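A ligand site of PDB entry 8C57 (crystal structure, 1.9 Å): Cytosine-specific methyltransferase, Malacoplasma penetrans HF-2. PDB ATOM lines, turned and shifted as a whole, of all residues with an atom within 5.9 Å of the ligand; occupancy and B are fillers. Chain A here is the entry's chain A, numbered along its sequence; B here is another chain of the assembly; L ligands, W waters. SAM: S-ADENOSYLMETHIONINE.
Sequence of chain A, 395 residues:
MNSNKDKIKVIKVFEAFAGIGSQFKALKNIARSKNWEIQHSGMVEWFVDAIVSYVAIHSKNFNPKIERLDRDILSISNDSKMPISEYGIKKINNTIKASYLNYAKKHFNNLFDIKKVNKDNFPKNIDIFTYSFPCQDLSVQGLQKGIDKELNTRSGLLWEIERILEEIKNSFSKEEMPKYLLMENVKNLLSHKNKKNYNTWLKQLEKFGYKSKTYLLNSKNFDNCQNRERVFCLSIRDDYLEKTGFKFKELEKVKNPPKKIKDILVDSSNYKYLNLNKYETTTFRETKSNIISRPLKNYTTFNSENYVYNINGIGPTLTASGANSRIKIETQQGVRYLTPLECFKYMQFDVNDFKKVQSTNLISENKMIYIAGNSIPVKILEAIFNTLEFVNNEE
Water W3 lies within hydrogen-bond range of an oxygen (OXT) of the ligand, the backbone carbonyl oxygen (O) of Ile 371 and the backbone NH (N) of Ile 20. Water W2 bridges an oxygen (O3') of the ligand (2.8 Å) and the side-chain amide nitrogen of Asn 374 (3.4 Å). Water W4 lies within hydrogen-bond range of OE1 of Glu 184 and N of the ligand.
O of Ala 18 sits close to O of the ligand. A nitrogen (N1) of the ligand lies close to the backbone carbonyl oxygen (O) of Phe 112 (3.2 Å). The backbone carbonyl oxygen (O) of Asn 374 sits close to a sulfur (SD) of the ligand. Merely in contact with the ligand: Phe 47 (3.2 Å), Phe 17 (3.2 Å), Gly 19 (3.5 Å), TJU 8 of chain B (3.5 Å), Ile 114 (3.5 Å), Gly 21 (3.6 Å), Val 44 (3.6 Å), Ile 376 (3.6 Å), Ser 80 (3.8 Å) and Leu 157 (3.98 Å).
OE2 of Glu 45 sits at hydrogen-bond distance from O2' of the ligand, 2.7 Å away. O of the ligand sits at hydrogen-bond distance from N of Ser 22. The side-chain hydroxyl (OG) of Ser 22 is in hydrogen-bond range of an oxygen (O) of the ligand (2.7 Å). An oxygen (OXT) of the ligand is in hydrogen-bond range of the side-chain hydroxyl (OG) of Ser 375 (3.0 Å). The backbone NH (N) of Ile 20 is in hydrogen-bond range of an oxygen (OXT) of the ligand (3.1 Å). OD1 of Asp 113 is in hydrogen-bond range of N6 of the ligand, 3.2 Å away. The backbone NH (N) of Trp 46 lies within hydrogen-bond range of a nitrogen (N3) of the ligand (3.5 Å). The side-chain amide nitrogen (NE2) of Gln 23 sits close to a nitrogen (N) of the ligand, at 3.4 Å.
The side-chain carboxylate (OE1) of Glu 45 lies within hydrogen-bond range of the backbone NH (N) of Ala 18 (3.4 Å). The backbone NH of Phe 47 is in hydrogen-bond range of the side-chain carboxylate of Glu 45, at 3.0 Å. N of Gly 19 lies within hydrogen-bond range of OE1 of Glu 45 (2.8 Å). The backbone carbonyl oxygen (O) of Phe 112 sits close to the backbone NH (N) of Trp 46 (3.3 Å). N of Lys 115 sits close to OD1 of Asp 113. The backbone carbonyl oxygen (O) of Val 44 lies within hydrogen-bond range of the backbone NH (N) of Phe 17, 2.7 Å away. The side-chain amide oxygen (OE1) of Gln 23 lies close to the side-chain carboxylate (OE2) of Glu 15 (3.1 Å). N4 of TJU 8 of chain B sits at hydrogen-bond distance from the side-chain hydroxyl (OG) of Ser 132, at 3.2 Å.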
ATOM      1  N   GLU A  15      23.439  23.450  -9.494  1.00  0.00           N
ATOM      2  CA  GLU A  15      23.559  23.778  -8.074  1.00  0.00           C
ATOM      3  C   GLU A  15      22.588  22.963  -7.238  1.00  0.00           C
ATOM      4  O   GLU A  15      21.398  23.264  -7.216  1.00  0.00           O
ATOM      5  CB  GLU A  15      23.262  25.267  -7.848  1.00  0.00           C
ATOM      6  CG  GLU A  15      24.258  26.239  -8.460  1.00  0.00           C
ATOM      7  CD  GLU A  15      23.761  27.666  -8.421  1.00  0.00           C
ATOM      8  OE1 GLU A  15      22.991  28.040  -9.344  1.00  0.00           O
ATOM      9  OE2 GLU A  15      24.139  28.415  -7.467  1.00  0.00           O
ATOM     10  N   PHE A  17      21.053  22.038  -3.715  1.00  0.00           N
ATOM     11  CA  PHE A  17      20.880  22.764  -2.454  1.00  0.00           C
ATOM     12  C   PHE A  17      21.409  24.190  -2.628  1.00  0.00           C
ATOM     13  O   PHE A  17      22.246  24.661  -1.868  1.00  0.00           O
ATOM     14  CB  PHE A  17      21.540  22.014  -1.300  1.00  0.00           C
ATOM     15  CG  PHE A  17      21.314  20.535  -1.353  1.00  0.00           C
ATOM     16  CD1 PHE A  17      20.033  20.023  -1.480  1.00  0.00           C
ATOM     17  CD2 PHE A  17      22.382  19.648  -1.297  1.00  0.00           C
ATOM     18  CE1 PHE A  17      19.823  18.656  -1.546  1.00  0.00           C
ATOM     19  CE2 PHE A  17      22.180  18.276  -1.374  1.00  0.00           C
ATOM     20  CZ  PHE A  17      20.898  17.787  -1.495  1.00  0.00           C
ATOM     21  N   ALA A  18      20.872  24.854  -3.649  1.00  0.00           N
ATOM     22  CA  ALA A  18      21.425  26.079  -4.187  1.00  0.00           C
ATOM     23  C   ALA A  18      21.281  27.313  -3.296  1.00  0.00           C
ATOM     24  O   ALA A  18      22.077  28.245  -3.432  1.00  0.00           O
ATOM     25  CB  ALA A  18      20.769  26.363  -5.540  1.00  0.00           C
ATOM     26  N   GLY A  19      20.285  27.332  -2.424  1.00  0.00           N
ATOM     27  CA  GLY A  19      20.001  28.507  -1.605  1.00  0.00           C
ATOM     28  C   GLY A  19      19.754  29.716  -2.494  1.00  0.00           C
ATOM     29  O   GLY A  19      18.956  29.653  -3.431  1.00  0.00           O
ATOM     30  N   ILE A  20      20.455  30.807  -2.205  1.00  0.00           N
ATOM     31  CA  ILE A  20      20.350  32.032  -3.013  1.00  0.00           C
ATOM     32  C   ILE A  20      21.429  32.102  -4.099  1.00  0.00           C
ATOM     33  O   ILE A  20      21.585  33.132  -4.751  1.00  0.00           O
ATOM     34  CB  ILE A  20      20.403  33.293  -2.123  1.00  0.00           C
ATOM     35  CG1 ILE A  20      21.636  33.306  -1.226  1.00  0.00           C
ATOM     36  CG2 ILE A  20      19.160  33.347  -1.265  1.00  0.00           C
ATOM     37  CD1 ILE A  20      21.874  34.638  -0.540  1.00  0.00           C
ATOM     38  N   GLY A  21      22.166  31.015  -4.288  1.00  0.00           N
ATOM     39  CA  GLY A  21      23.078  30.910  -5.420  1.00  0.00           C
ATOM     40  C   GLY A  21      24.395  31.650  -5.261  1.00  0.00           C
ATOM     41  O   GLY A  21      24.799  32.377  -6.165  1.00  0.00           O
ATOM     42  N   SER A  22      25.053  31.517  -4.102  1.00  0.00           N
ATOM     43  CA  SER A  22      26.361  32.157  -3.911  1.00  0.00           C
ATOM     44  C   SER A  22      27.328  31.674  -4.988  1.00  0.00           C
ATOM     45  O   SER A  22      28.165  32.418  -5.493  1.00  0.00           O
ATOM     46  CB  SER A  22      26.928  31.815  -2.536  1.00  0.00           C
ATOM     47  OG  SER A  22      27.009  30.411  -2.347  1.00  0.00           O
ATOM     48  N   GLN A  23      27.184  30.390  -5.327  1.00  0.00           N
ATOM     49  CA  GLN A  23      27.992  29.711  -6.344  1.00  0.00           C
ATOM     50  C   GLN A  23      27.837  30.320  -7.735  1.00  0.00           C
ATOM     51  O   GLN A  23      28.819  30.665  -8.379  1.00  0.00           O
ATOM     52  CB  GLN A  23      27.651  28.220  -6.420  1.00  0.00           C
ATOM     53  CG  GLN A  23      27.817  27.449  -5.122  1.00  0.00           C
ATOM     54  CD  GLN A  23      26.525  27.303  -4.342  1.00  0.00           C
ATOM     55  OE1 GLN A  23      25.493  27.881  -4.682  1.00  0.00           O
ATOM     56  NE2 GLN A  23      26.575  26.496  -3.298  1.00  0.00           N
ATOM     57  N   VAL A  44      18.659  22.446  -7.566  1.00  0.00           N
ATOM     58  CA  VAL A  44      17.767  21.774  -6.646  1.00  0.00           C
ATOM     59  C   VAL A  44      17.664  22.636  -5.391  1.00  0.00           C
ATOM     60  O   VAL A  44      18.655  22.817  -4.678  1.00  0.00           O
ATOM     61  CB  VAL A  44      18.270  20.364  -6.299  1.00  0.00           C
ATOM     62  CG1 VAL A  44      17.279  19.623  -5.424  1.00  0.00           C
ATOM     63  CG2 VAL A  44      18.548  19.579  -7.572  1.00  0.00           C
ATOM     64  N   GLU A  45      16.494  23.205  -5.156  1.00  0.00           N
ATOM     65  CA  GLU A  45      16.241  23.983  -3.956  1.00  0.00           C
ATOM     66  C   GLU A  45      14.748  23.962  -3.686  1.00  0.00           C
ATOM     67  O   GLU A  45      13.952  24.317  -4.550  1.00  0.00           O
ATOM     68  CB  GLU A  45      16.736  25.427  -4.118  1.00  0.00           C
ATOM     69  CG  GLU A  45      16.538  26.300  -2.893  1.00  0.00           C
ATOM     70  CD  GLU A  45      17.074  25.653  -1.629  1.00  0.00           C
ATOM     71  OE1 GLU A  45      18.311  25.496  -1.531  1.00  0.00           O
ATOM     72  OE2 GLU A  45      16.263  25.270  -0.755  1.00  0.00           O
ATOM     73  N   TRP A  46      14.371  23.533  -2.483  1.00  0.00           N
ATOM     74  CA  TRP A  46      12.956  23.407  -2.141  1.00  0.00           C
ATOM     75  C   TRP A  46      12.416  24.456  -1.191  1.00  0.00           C
ATOM     76  O   TRP A  46      11.217  24.484  -0.940  1.00  0.00           O
ATOM     77  CB  TRP A  46      12.679  22.013  -1.587  1.00  0.00           C
ATOM     78  CG  TRP A  46      12.992  21.808  -0.141  1.00  0.00           C
ATOM     79  CD1 TRP A  46      13.942  22.439   0.603  1.00  0.00           C
ATOM     80  CD2 TRP A  46      12.370  20.863   0.723  1.00  0.00           C
ATOM     81  NE1 TRP A  46      13.922  21.968   1.889  1.00  0.00           N
ATOM     82  CE2 TRP A  46      12.969  20.981   1.985  1.00  0.00           C
ATOM     83  CE3 TRP A  46      11.336  19.922   0.553  1.00  0.00           C
ATOM     84  CZ2 TRP A  46      12.586  20.204   3.081  1.00  0.00           C
ATOM     85  CZ3 TRP A  46      10.965  19.148   1.637  1.00  0.00           C
ATOM     86  CH2 TRP A  46      11.579  19.302   2.890  1.00  0.00           C
ATOM     87  N   PHE A  47      13.301  25.286  -0.651  1.00  0.00           N
ATOM     88  CA  PHE A  47      12.937  26.278   0.369  1.00  0.00           C
ATOM     89  C   PHE A  47      12.358  27.508  -0.335  1.00  0.00           C
ATOM     90  O   PHE A  47      13.059  28.217  -1.030  1.00  0.00           O
ATOM     91  CB  PHE A  47      14.186  26.611   1.192  1.00  0.00           C
ATOM     92  CG  PHE A  47      14.000  27.654   2.269  1.00  0.00           C
ATOM     93  CD1 PHE A  47      12.799  27.828   2.924  1.00  0.00           C
ATOM     94  CD2 PHE A  47      15.111  28.390   2.684  1.00  0.00           C
ATOM     95  CE1 PHE A  47      12.668  28.782   3.919  1.00  0.00           C
ATOM     96  CE2 PHE A  47      14.991  29.343   3.698  1.00  0.00           C
ATOM     97  CZ  PHE A  47      13.774  29.536   4.310  1.00  0.00           C
ATOM     98  N   ALA A  50      14.167  30.925  -0.277  1.00  0.00           N
ATOM     99  CA  ALA A  50      15.427  30.869  -1.025  1.00  0.00           C
ATOM    100  C   ALA A  50      15.166  30.901  -2.537  1.00  0.00           C
ATOM    101  O   ALA A  50      15.892  31.547  -3.264  1.00  0.00           O
ATOM    102  CB  ALA A  50      16.210  29.622  -0.665  1.00  0.00           C
ATOM    103  N   SER A  80      12.258  25.339   5.329  1.00  0.00           N
ATOM    104  CA  SER A  80      13.514  24.724   4.834  1.00  0.00           C
ATOM    105  C   SER A  80      13.786  23.309   5.390  1.00  0.00           C
ATOM    106  O   SER A  80      14.638  22.599   4.855  1.00  0.00           O
ATOM    107  CB  SER A  80      14.752  25.625   5.056  1.00  0.00           C
ATOM    108  OG  SER A  80      15.336  25.431   6.339  1.00  0.00           O
ATOM    109  N   PHE A 112      13.734  21.044  -7.597  1.00  0.00           N
ATOM    110  CA  PHE A 112      13.137  21.244  -6.259  1.00  0.00           C
ATOM    111  C   PHE A 112      13.598  20.297  -5.163  1.00  0.00           C
ATOM    112  O   PHE A 112      14.142  20.744  -4.152  1.00  0.00           O
ATOM    113  CB  PHE A 112      11.609  21.285  -6.335  1.00  0.00           C
ATOM    114  CG  PHE A 112      11.090  22.461  -7.108  1.00  0.00           C
ATOM    115  CD1 PHE A 112      10.907  23.688  -6.488  1.00  0.00           C
ATOM    116  CD2 PHE A 112      10.807  22.351  -8.467  1.00  0.00           C
ATOM    117  CE1 PHE A 112      10.441  24.778  -7.200  1.00  0.00           C
ATOM    118  CE2 PHE A 112      10.332  23.445  -9.178  1.00  0.00           C
ATOM    119  CZ  PHE A 112      10.156  24.661  -8.547  1.00  0.00           C
ATOM    120  N   ASP A 113      13.390  18.999  -5.356  1.00  0.00           N
ATOM    121  CA  ASP A 113      13.665  18.011  -4.339  1.00  0.00           C
ATOM    122  C   ASP A 113      14.670  17.006  -4.900  1.00  0.00           C
ATOM    123  O   ASP A 113      14.449  16.429  -5.970  1.00  0.00           O
ATOM    124  CB  ASP A 113      12.347  17.309  -3.993  1.00  0.00           C
ATOM    125  CG  ASP A 113      12.454  16.368  -2.808  1.00  0.00           C
ATOM    126  OD1 ASP A 113      13.564  16.074  -2.317  1.00  0.00           O
ATOM    127  OD2 ASP A 113      11.378  15.908  -2.376  1.00  0.00           O
ATOM    128  N   ILE A 114      15.770  16.810  -4.170  1.00  0.00           N
ATOM    129  CA  ILE A 114      16.831  15.915  -4.604  1.00  0.00           C
ATOM    130  C   ILE A 114      16.355  14.458  -4.812  1.00  0.00           C
ATOM    131  O   ILE A 114      16.883  13.770  -5.676  1.00  0.00           O
ATOM    132  CB  ILE A 114      18.037  15.957  -3.637  1.00  0.00           C
ATOM    133  CG1 ILE A 114      19.282  15.360  -4.298  1.00  0.00           C
ATOM    134  CG2 ILE A 114      17.722  15.260  -2.328  1.00  0.00           C
ATOM    135  CD1 ILE A 114      19.880  16.228  -5.380  1.00  0.00           C
ATOM    136  N   LYS A 115      15.361  14.023  -4.057  1.00  0.00           N
ATOM    137  CA  LYS A 115      14.805  12.672  -4.203  1.00  0.00           C
ATOM    138  C   LYS A 115      14.089  12.496  -5.541  1.00  0.00           C
ATOM    139  O   LYS A 115      13.884  11.362  -6.002  1.00  0.00           O
ATOM    140  CB  LYS A 115      13.860  12.351  -3.046  1.00  0.00           C
ATOM    141  CG  LYS A 115      14.456  12.651  -1.685  1.00  0.00           C
ATOM    142  CD  LYS A 115      13.558  12.143  -0.570  1.00  0.00           C
ATOM    143  CE  LYS A 115      14.185  12.364   0.792  1.00  0.00           C
ATOM    144  NZ  LYS A 115      13.443  11.618   1.850  1.00  0.00           N
ATOM    145  N   SER A 132      26.191  19.884  -1.093  1.00  0.00           N
ATOM    146  CA  SER A 132      26.537  19.880   0.319  1.00  0.00           C
ATOM    147  C   SER A 132      25.729  18.761   0.975  1.00  0.00           C
ATOM    148  O   SER A 132      24.996  18.044   0.300  1.00  0.00           O
ATOM    149  CB  SER A 132      26.221  21.226   0.965  1.00  0.00           C
ATOM    150  OG  SER A 132      26.591  21.234   2.332  1.00  0.00           O
ATOM    151  N   LEU A 157      20.467  13.175   2.457  1.00  0.00           N
ATOM    152  CA  LEU A 157      20.774  13.919   1.233  1.00  0.00           C
ATOM    153  C   LEU A 157      22.004  13.370   0.514  1.00  0.00           C
ATOM    154  O   LEU A 157      22.033  13.359  -0.722  1.00  0.00           O
ATOM    155  CB  LEU A 157      20.995  15.408   1.542  1.00  0.00           C
ATOM    156  CG  LEU A 157      19.775  16.328   1.624  1.00  0.00           C
ATOM    157  CD1 LEU A 157      18.578  15.666   2.286  1.00  0.00           C
ATOM    158  CD2 LEU A 157      20.151  17.626   2.318  1.00  0.00           C
ATOM    159  N   GLU A 184      30.579  22.187  -0.300  1.00  0.00           N
ATOM    160  CA  GLU A 184      30.844  23.053   0.843  1.00  0.00           C
ATOM    161  C   GLU A 184      30.262  22.380   2.059  1.00  0.00           C
ATOM    162  O   GLU A 184      29.265  21.665   1.964  1.00  0.00           O
ATOM    163  CB  GLU A 184      30.194  24.434   0.664  1.00  0.00           C
ATOM    164  CG  GLU A 184      30.313  25.358   1.877  1.00  0.00           C
ATOM    165  CD  GLU A 184      29.105  25.308   2.823  1.00  0.00           C
ATOM    166  OE1 GLU A 184      28.160  24.530   2.569  1.00  0.00           O
ATOM    167  OE2 GLU A 184      29.106  26.062   3.828  1.00  0.00           O
ATOM    168  N   PHE A 349      27.698  39.242  -1.025  1.00  0.00           N
ATOM    169  CA  PHE A 349      26.734  39.632  -2.037  1.00  0.00           C
ATOM    170  C   PHE A 349      26.786  41.153  -2.112  1.00  0.00           C
ATOM    171  O   PHE A 349      27.302  41.797  -1.208  1.00  0.00           O
ATOM    172  CB  PHE A 349      25.333  39.137  -1.678  1.00  0.00           C
ATOM    173  CG  PHE A 349      25.153  37.660  -1.912  1.00  0.00           C
ATOM    174  CD1 PHE A 349      25.575  36.743  -0.981  1.00  0.00           C
ATOM    175  CD2 PHE A 349      24.585  37.203  -3.092  1.00  0.00           C
ATOM    176  CE1 PHE A 349      25.415  35.384  -1.200  1.00  0.00           C
ATOM    177  CE2 PHE A 349      24.433  35.838  -3.321  1.00  0.00           C
ATOM    178  CZ  PHE A 349      24.839  34.933  -2.370  1.00  0.00           C
ATOM    179  N   ILE A 371      18.506  33.248   5.082  1.00  0.00           N
ATOM    180  CA  ILE A 371      19.060  32.792   3.810  1.00  0.00           C
ATOM    181  C   ILE A 371      20.513  33.234   3.638  1.00  0.00           C
ATOM    182  O   ILE A 371      21.314  32.485   3.078  1.00  0.00           O
ATOM    183  CB  ILE A 371      18.165  33.143   2.580  1.00  0.00           C
ATOM    184  CG1 ILE A 371      18.028  34.646   2.380  1.00  0.00           C
ATOM    185  CG2 ILE A 371      16.778  32.552   2.761  1.00  0.00           C
ATOM    186  CD1 ILE A 371      17.004  35.029   1.326  1.00  0.00           C
ATOM    187  N   ASN A 374      22.743  30.897   5.707  1.00  0.00           N
ATOM    188  CA  ASN A 374      22.917  29.604   5.029  1.00  0.00           C
ATOM    189  C   ASN A 374      23.817  29.610   3.784  1.00  0.00           C
ATOM    190  O   ASN A 374      24.131  28.543   3.269  1.00  0.00           O
ATOM    191  CB  ASN A 374      21.543  29.042   4.596  1.00  0.00           C
ATOM    192  CG  ASN A 374      20.812  28.365   5.721  1.00  0.00           C
ATOM    193  OD1 ASN A 374      21.401  27.669   6.525  1.00  0.00           O
ATOM    194  ND2 ASN A 374      19.509  28.530   5.765  1.00  0.00           N
ATOM    195  N   SER A 375      24.234  30.789   3.324  1.00  0.00           N
ATOM    196  CA  SER A 375      24.986  30.882   2.083  1.00  0.00           C
ATOM    197  C   SER A 375      26.494  30.701   2.323  1.00  0.00           C
ATOM    198  O   SER A 375      26.917  30.315   3.408  1.00  0.00           O
ATOM    199  CB  SER A 375      24.700  32.203   1.394  1.00  0.00           C
ATOM    200  OG  SER A 375      25.019  32.122   0.020  1.00  0.00           O
ATOM    201  N   ILE A 376      27.281  30.973   1.279  1.00  0.00           N
ATOM    202  CA  ILE A 376      28.737  30.846   1.330  1.00  0.00           C
ATOM    203  C   ILE A 376      29.346  32.181   0.927  1.00  0.00           C
ATOM    204  O   ILE A 376      28.910  32.775  -0.064  1.00  0.00           O
ATOM    205  CB  ILE A 376      29.204  29.790   0.319  1.00  0.00           C
ATOM    206  CG1 ILE A 376      28.430  28.475   0.525  1.00  0.00           C
ATOM    207  CG2 ILE A 376      30.714  29.606   0.415  1.00  0.00           C
ATOM    208  CD1 ILE A 376      28.617  27.465  -0.600  1.00  0.00           C
ATOM    209  C2  TJU B   8      26.663  26.717   6.194  1.00  0.00           C
ATOM    210  C4  TJU B   8      26.136  24.586   5.435  1.00  0.00           C
ATOM    211  C5  TJU B   8      24.122  23.357   6.318  1.00  0.00           C
ATOM    212  C6  TJU B   8      25.119  25.286   7.515  1.00  0.00           C
ATOM    213  O2  TJU B   8      27.386  27.695   6.163  1.00  0.00           O
ATOM    214  N3  TJU B   8      26.940  25.627   5.391  1.00  0.00           N
ATOM    215  N4  TJU B   8      26.416  23.559   4.578  1.00  0.00           N
ATOM    216  N5  TJU B   8      25.192  24.363   6.409  1.00  0.00           N
ATOM    217  N1  TJU B   8      25.540  26.622   7.065  1.00  0.00           N
ATOM    218  C1' TJU B   8      25.308  27.754   7.978  1.00  0.00           C
ATOM    219  O4' TJU B   8      26.285  27.588   9.017  1.00  0.00           O
ATOM    220  C2' TJU B   8      23.940  27.798   8.629  1.00  0.00           C
ATOM    221  C3' TJU B   8      24.221  27.443  10.088  1.00  0.00           C
ATOM    222  O3' TJU B   8      23.416  28.244  10.978  1.00  0.00           O
ATOM    223  C4' TJU B   8      25.657  27.932  10.249  1.00  0.00           C
ATOM    224  C5' TJU B   8      26.385  27.173  11.303  1.00  0.00           C
ATOM    225  O5' TJU B   8      27.658  27.839  11.452  1.00  0.00           O
ATOM    226  P   TJU B   8      28.913  27.048  12.204  1.00  0.00           P
ATOM    227  OP2 TJU B   8      28.693  25.603  12.164  1.00  0.00           O
ATOM    228  OP1 TJU B   8      30.157  27.629  11.654  1.00  0.00           O
HETATM  229  N   SAM L   1      24.974  27.438  -0.404  1.00  0.00           N
HETATM  230  CA  SAM L   1      23.586  27.856  -0.562  1.00  0.00           C
HETATM  231  C   SAM L   1      23.608  29.322  -0.951  1.00  0.00           C
HETATM  232  O   SAM L   1      24.415  29.695  -1.823  1.00  0.00           O
HETATM  233  OXT SAM L   1      22.838  30.143  -0.409  1.00  0.00           O
HETATM  234  CB  SAM L   1      22.744  27.511   0.678  1.00  0.00           C
HETATM  235  CG  SAM L   1      23.026  26.097   1.211  1.00  0.00           C
HETATM  236  SD  SAM L   1      22.009  25.626   2.449  1.00  0.00           S
HETATM  237  CE  SAM L   1      22.909  25.518   3.857  1.00  0.00           C
HETATM  238  C5' SAM L   1      21.321  24.145   2.141  1.00  0.00           C
HETATM  239  C4' SAM L   1      20.005  24.278   1.370  1.00  0.00           C
HETATM  240  O4' SAM L   1      19.525  22.980   0.988  1.00  0.00           O
HETATM  241  C3' SAM L   1      18.893  24.935   2.187  1.00  0.00           C
HETATM  242  O3' SAM L   1      18.553  26.221   1.625  1.00  0.00           O
HETATM  243  C2' SAM L   1      17.733  23.944   2.137  1.00  0.00           C
HETATM  244  O2' SAM L   1      16.510  24.580   1.842  1.00  0.00           O
HETATM  245  C1' SAM L   1      18.101  23.000   1.005  1.00  0.00           C
HETATM  246  N9  SAM L   1      17.511  21.641   1.122  1.00  0.00           N
HETATM  247  C8  SAM L   1      17.394  20.824   2.201  1.00  0.00           C
HETATM  248  N7  SAM L   1      16.767  19.662   1.843  1.00  0.00           N
HETATM  249  C5  SAM L   1      16.470  19.738   0.533  1.00  0.00           C
HETATM  250  C6  SAM L   1      15.829  18.873  -0.486  1.00  0.00           C
HETATM  251  N6  SAM L   1      15.327  17.644  -0.190  1.00  0.00           N
HETATM  252  N1  SAM L   1      15.743  19.350  -1.749  1.00  0.00           N
HETATM  253  C2  SAM L   1      16.218  20.571  -2.081  1.00  0.00           C
HETATM  254  N3  SAM L   1      16.803  21.400  -1.211  1.00  0.00           N
HETATM  255  C4  SAM L   1      16.959  21.031   0.072  1.00  0.00           C
HETATM  256  O   HOH W   1      12.968  16.071   1.804  1.00  0.00           O
HETATM  257  O   HOH W   2      18.632  28.913   2.481  1.00  0.00           O
HETATM  258  O   HOH W   3      20.808  30.454   1.248  1.00  0.00           O
HETATM  259  O   HOH W   4      26.298  24.562   0.341  1.00  0.00           O
